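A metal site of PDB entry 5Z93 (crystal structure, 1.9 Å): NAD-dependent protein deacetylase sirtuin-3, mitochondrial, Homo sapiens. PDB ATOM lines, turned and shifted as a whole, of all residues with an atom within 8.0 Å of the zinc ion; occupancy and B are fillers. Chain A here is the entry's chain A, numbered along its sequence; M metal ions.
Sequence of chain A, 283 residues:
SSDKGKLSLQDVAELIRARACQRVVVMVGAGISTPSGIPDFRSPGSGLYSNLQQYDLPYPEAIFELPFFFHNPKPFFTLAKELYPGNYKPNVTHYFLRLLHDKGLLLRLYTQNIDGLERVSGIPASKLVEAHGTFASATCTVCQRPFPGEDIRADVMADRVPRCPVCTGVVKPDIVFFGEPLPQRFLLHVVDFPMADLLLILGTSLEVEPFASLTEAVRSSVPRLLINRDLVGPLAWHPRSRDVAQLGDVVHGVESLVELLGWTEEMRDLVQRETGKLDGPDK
SG of Cys 167 sits close to N of Gly 169 (3.4 Å). SG of Cys 143 sits close to NH2 of Arg 145 (3.3 Å). The backbone NH of Cys 164 is in hydrogen-bond range of the backbone carbonyl oxygen of Gly 169, at 2.6 Å. N of Val 166 sits close to SG of Cys 164 (3.4 Å). The side-chain sulfur of Cys 140 sits close to the backbone NH of Val 142 (3.3 Å). O of Arg 145 lies within hydrogen-bond range of N of Cys 140 (2.8 Å).
The zinc ion is bound by SG of Cys 167, SG of Cys 143, SG of Cys 164 and SG of Cys 140.
The nearest printed residue that does not touch the zinc ion is Gly 169 (4.6 Å).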
ATOM      1  N   THR A 139      18.906 -15.141   8.577  1.00  0.00           N
ATOM      2  CA  THR A 139      19.469 -14.717   9.850  1.00  0.00           C
ATOM      3  C   THR A 139      19.112 -15.730  10.931  1.00  0.00           C
ATOM      4  O   THR A 139      17.941 -16.112  11.063  1.00  0.00           O
ATOM      5  CB  THR A 139      18.953 -13.322  10.247  1.00  0.00           C
ATOM      6  OG1 THR A 139      19.308 -12.398   9.222  1.00  0.00           O
ATOM      7  CG2 THR A 139      19.569 -12.853  11.563  1.00  0.00           C
ATOM      8  N   CYS A 140      20.099 -16.154  11.719  1.00  0.00           N
ATOM      9  CA  CYS A 140      19.817 -17.044  12.834  1.00  0.00           C
ATOM     10  C   CYS A 140      18.897 -16.367  13.843  1.00  0.00           C
ATOM     11  O   CYS A 140      19.148 -15.225  14.238  1.00  0.00           O
ATOM     12  CB  CYS A 140      21.113 -17.482  13.508  1.00  0.00           C
ATOM     13  SG  CYS A 140      20.771 -18.524  14.926  1.00  0.00           S
ATOM     14  N   THR A 141      17.820 -17.038  14.254  1.00  0.00           N
ATOM     15  CA  THR A 141      16.901 -16.428  15.208  1.00  0.00           C
ATOM     16  C   THR A 141      17.448 -16.371  16.629  1.00  0.00           C
ATOM     17  O   THR A 141      16.852 -15.691  17.471  1.00  0.00           O
ATOM     18  CB  THR A 141      15.562 -17.162  15.241  1.00  0.00           C
ATOM     19  OG1 THR A 141      15.786 -18.527  15.571  1.00  0.00           O
ATOM     20  CG2 THR A 141      14.852 -17.078  13.896  1.00  0.00           C
ATOM     21  N   VAL A 142      18.533 -17.064  16.922  1.00  0.00           N
ATOM     22  CA  VAL A 142      19.077 -17.115  18.283  1.00  0.00           C
ATOM     23  C   VAL A 142      20.290 -16.206  18.439  1.00  0.00           C
ATOM     24  O   VAL A 142      20.332 -15.371  19.341  1.00  0.00           O
ATOM     25  CB  VAL A 142      19.399 -18.565  18.685  1.00  0.00           C
ATOM     26  CG1 VAL A 142      20.098 -18.616  20.061  1.00  0.00           C
ATOM     27  CG2 VAL A 142      18.138 -19.387  18.723  1.00  0.00           C
ATOM     28  N   CYS A 143      21.260 -16.322  17.528  1.00  0.00           N
ATOM     29  CA  CYS A 143      22.492 -15.545  17.640  1.00  0.00           C
ATOM     30  C   CYS A 143      22.600 -14.392  16.649  1.00  0.00           C
ATOM     31  O   CYS A 143      23.563 -13.619  16.729  1.00  0.00           O
ATOM     32  CB  CYS A 143      23.715 -16.474  17.478  1.00  0.00           C
ATOM     33  SG  CYS A 143      24.077 -17.056  15.803  1.00  0.00           S
ATOM     34  N   GLN A 144      21.654 -14.245  15.710  1.00  0.00           N
ATOM     35  CA  GLN A 144      21.576 -13.156  14.737  1.00  0.00           C
ATOM     36  C   GLN A 144      22.684 -13.177  13.678  1.00  0.00           C
ATOM     37  O   GLN A 144      22.836 -12.205  12.937  1.00  0.00           O
ATOM     38  CB  GLN A 144      21.565 -11.776  15.426  1.00  0.00           C
ATOM     39  CG  GLN A 144      20.396 -11.606  16.417  1.00  0.00           C
ATOM     40  CD  GLN A 144      19.040 -11.730  15.754  1.00  0.00           C
ATOM     41  OE1 GLN A 144      18.810 -11.177  14.675  1.00  0.00           O
ATOM     42  NE2 GLN A 144      18.124 -12.450  16.394  1.00  0.00           N
ATOM     43  N   ARG A 145      23.451 -14.267  13.573  1.00  0.00           N
ATOM     44  CA  ARG A 145      24.398 -14.384  12.470  1.00  0.00           C
ATOM     45  C   ARG A 145      23.647 -14.410  11.132  1.00  0.00           C
ATOM     46  O   ARG A 145      22.620 -15.082  11.006  1.00  0.00           O
ATOM     47  CB  ARG A 145      25.217 -15.658  12.593  1.00  0.00           C
ATOM     48  CG  ARG A 145      26.429 -15.495  13.479  1.00  0.00           C
ATOM     49  CD  ARG A 145      27.128 -16.825  13.725  1.00  0.00           C
ATOM     50  NE  ARG A 145      28.341 -16.636  14.517  1.00  0.00           N
ATOM     51  CZ  ARG A 145      28.358 -16.481  15.831  1.00  0.00           C
ATOM     52  NH1 ARG A 145      29.512 -16.305  16.464  1.00  0.00           N
ATOM     53  NH2 ARG A 145      27.240 -16.484  16.524  1.00  0.00           N
ATOM     54  N   PRO A 146      24.165 -13.733  10.111  1.00  0.00           N
ATOM     55  CA  PRO A 146      23.566 -13.797   8.770  1.00  0.00           C
ATOM     56  C   PRO A 146      24.222 -14.845   7.883  1.00  0.00           C
ATOM     57  O   PRO A 146      25.377 -15.224   8.081  1.00  0.00           O
ATOM     58  CB  PRO A 146      23.819 -12.382   8.227  1.00  0.00           C
ATOM     59  CG  PRO A 146      25.173 -12.040   8.819  1.00  0.00           C
ATOM     60  CD  PRO A 146      25.244 -12.727  10.176  1.00  0.00           C
ATOM     61  N   PHE A 147      23.456 -15.307   6.906  1.00  0.00           N
ATOM     62  CA  PHE A 147      23.910 -16.304   5.960  1.00  0.00           C
ATOM     63  C   PHE A 147      23.336 -15.964   4.599  1.00  0.00           C
ATOM     64  O   PHE A 147      22.253 -15.370   4.513  1.00  0.00           O
ATOM     65  CB  PHE A 147      23.449 -17.717   6.355  1.00  0.00           C
ATOM     66  CG  PHE A 147      23.886 -18.128   7.739  1.00  0.00           C
ATOM     67  CD1 PHE A 147      25.121 -18.712   7.947  1.00  0.00           C
ATOM     68  CD2 PHE A 147      23.051 -17.896   8.837  1.00  0.00           C
ATOM     69  CE1 PHE A 147      25.544 -19.074   9.227  1.00  0.00           C
ATOM     70  CE2 PHE A 147      23.452 -18.258  10.110  1.00  0.00           C
ATOM     71  CZ  PHE A 147      24.702 -18.850  10.315  1.00  0.00           C
ATOM     72  N   ARG A 163      19.293 -25.132  10.579  1.00  0.00           N
ATOM     73  CA  ARG A 163      19.797 -24.765  11.887  1.00  0.00           C
ATOM     74  C   ARG A 163      21.174 -24.133  11.783  1.00  0.00           C
ATOM     75  O   ARG A 163      21.938 -24.411  10.862  1.00  0.00           O
ATOM     76  CB  ARG A 163      19.823 -25.982  12.817  1.00  0.00           C
ATOM     77  CG  ARG A 163      18.379 -26.467  13.117  1.00  0.00           C
ATOM     78  CD  ARG A 163      18.220 -27.045  14.497  1.00  0.00           C
ATOM     79  NE  ARG A 163      16.823 -27.261  14.858  1.00  0.00           N
ATOM     80  CZ  ARG A 163      16.190 -26.598  15.820  1.00  0.00           C
ATOM     81  NH1 ARG A 163      16.826 -25.676  16.529  1.00  0.00           N
ATOM     82  NH2 ARG A 163      14.913 -26.872  16.092  1.00  0.00           N
ATOM     83  N   CYS A 164      21.444 -23.223  12.714  1.00  0.00           N
ATOM     84  CA  CYS A 164      22.656 -22.417  12.680  1.00  0.00           C
ATOM     85  C   CYS A 164      23.875 -23.320  12.871  1.00  0.00           C
ATOM     86  O   CYS A 164      23.865 -24.175  13.762  1.00  0.00           O
ATOM     87  CB  CYS A 164      22.603 -21.353  13.778  1.00  0.00           C
ATOM     88  SG  CYS A 164      24.018 -20.211  13.875  1.00  0.00           S
ATOM     89  N   PRO A 165      24.915 -23.191  12.036  1.00  0.00           N
ATOM     90  CA  PRO A 165      26.144 -23.969  12.270  1.00  0.00           C
ATOM     91  C   PRO A 165      26.848 -23.625  13.573  1.00  0.00           C
ATOM     92  O   PRO A 165      27.634 -24.441  14.059  1.00  0.00           O
ATOM     93  CB  PRO A 165      27.020 -23.614  11.058  1.00  0.00           C
ATOM     94  CG  PRO A 165      26.076 -23.121  10.040  1.00  0.00           C
ATOM     95  CD  PRO A 165      24.932 -22.475  10.753  1.00  0.00           C
ATOM     96  N   VAL A 166      26.588 -22.457  14.157  1.00  0.00           N
ATOM     97  CA  VAL A 166      27.260 -22.040  15.377  1.00  0.00           C
ATOM     98  C   VAL A 166      26.462 -22.399  16.625  1.00  0.00           C
ATOM     99  O   VAL A 166      26.984 -23.009  17.557  1.00  0.00           O
ATOM    100  CB  VAL A 166      27.554 -20.516  15.314  1.00  0.00           C
ATOM    101  CG1 VAL A 166      28.119 -20.038  16.654  1.00  0.00           C
ATOM    102  CG2 VAL A 166      28.502 -20.192  14.166  1.00  0.00           C
ATOM    103  N   CYS A 167      25.180 -22.023  16.697  1.00  0.00           N
ATOM    104  CA  CYS A 167      24.411 -22.216  17.919  1.00  0.00           C
ATOM    105  C   CYS A 167      23.284 -23.232  17.799  1.00  0.00           C
ATOM    106  O   CYS A 167      22.629 -23.524  18.817  1.00  0.00           O
ATOM    107  CB  CYS A 167      23.827 -20.881  18.402  1.00  0.00           C
ATOM    108  SG  CYS A 167      22.451 -20.222  17.393  1.00  0.00           S
ATOM    109  N   THR A 168      23.041 -23.775  16.611  1.00  0.00           N
ATOM    110  CA  THR A 168      21.972 -24.739  16.286  1.00  0.00           C
ATOM    111  C   THR A 168      20.585 -24.114  16.325  1.00  0.00           C
ATOM    112  O   THR A 168      19.583 -24.830  16.180  1.00  0.00           O
ATOM    113  CB  THR A 168      21.989 -26.003  17.158  1.00  0.00           C
ATOM    114  OG1 THR A 168      21.463 -25.716  18.456  1.00  0.00           O
ATOM    115  CG2 THR A 168      23.415 -26.554  17.309  1.00  0.00           C
ATOM    116  N   GLY A 169      20.479 -22.791  16.482  1.00  0.00           N
ATOM    117  CA  GLY A 169      19.186 -22.145  16.403  1.00  0.00           C
ATOM    118  C   GLY A 169      18.609 -22.190  15.000  1.00  0.00           C
ATOM    119  O   GLY A 169      19.304 -22.391  14.006  1.00  0.00           O
ATOM    120  N   VAL A 170      17.290 -22.013  14.914  1.00  0.00           N
ATOM    121  CA  VAL A 170      16.615 -22.013  13.619  1.00  0.00           C
ATOM    122  C   VAL A 170      17.016 -20.774  12.822  1.00  0.00           C
ATOM    123  O   VAL A 170      16.946 -19.644  13.308  1.00  0.00           O
ATOM    124  CB  VAL A 170      15.095 -22.070  13.819  1.00  0.00           C
ATOM    125  CG1 VAL A 170      14.374 -21.854  12.482  1.00  0.00           C
ATOM    126  CG2 VAL A 170      14.695 -23.420  14.379  1.00  0.00           C
ATOM    127  N   VAL A 171      17.428 -20.997  11.593  1.00  0.00           N
ATOM    128  CA  VAL A 171      17.801 -19.894  10.714  1.00  0.00           C
ATOM    129  C   VAL A 171      16.584 -19.508   9.878  1.00  0.00           C
ATOM    130  O   VAL A 171      15.955 -20.371   9.260  1.00  0.00           O
ATOM    131  CB  VAL A 171      18.986 -20.294   9.805  1.00  0.00           C
ATOM    132  CG1 VAL A 171      19.288 -19.169   8.829  1.00  0.00           C
ATOM    133  CG2 VAL A 171      20.205 -20.636  10.675  1.00  0.00           C
HETATM  134 ZN    ZN M   1      22.999 -19.055  15.562  1.00  0.00          ZN
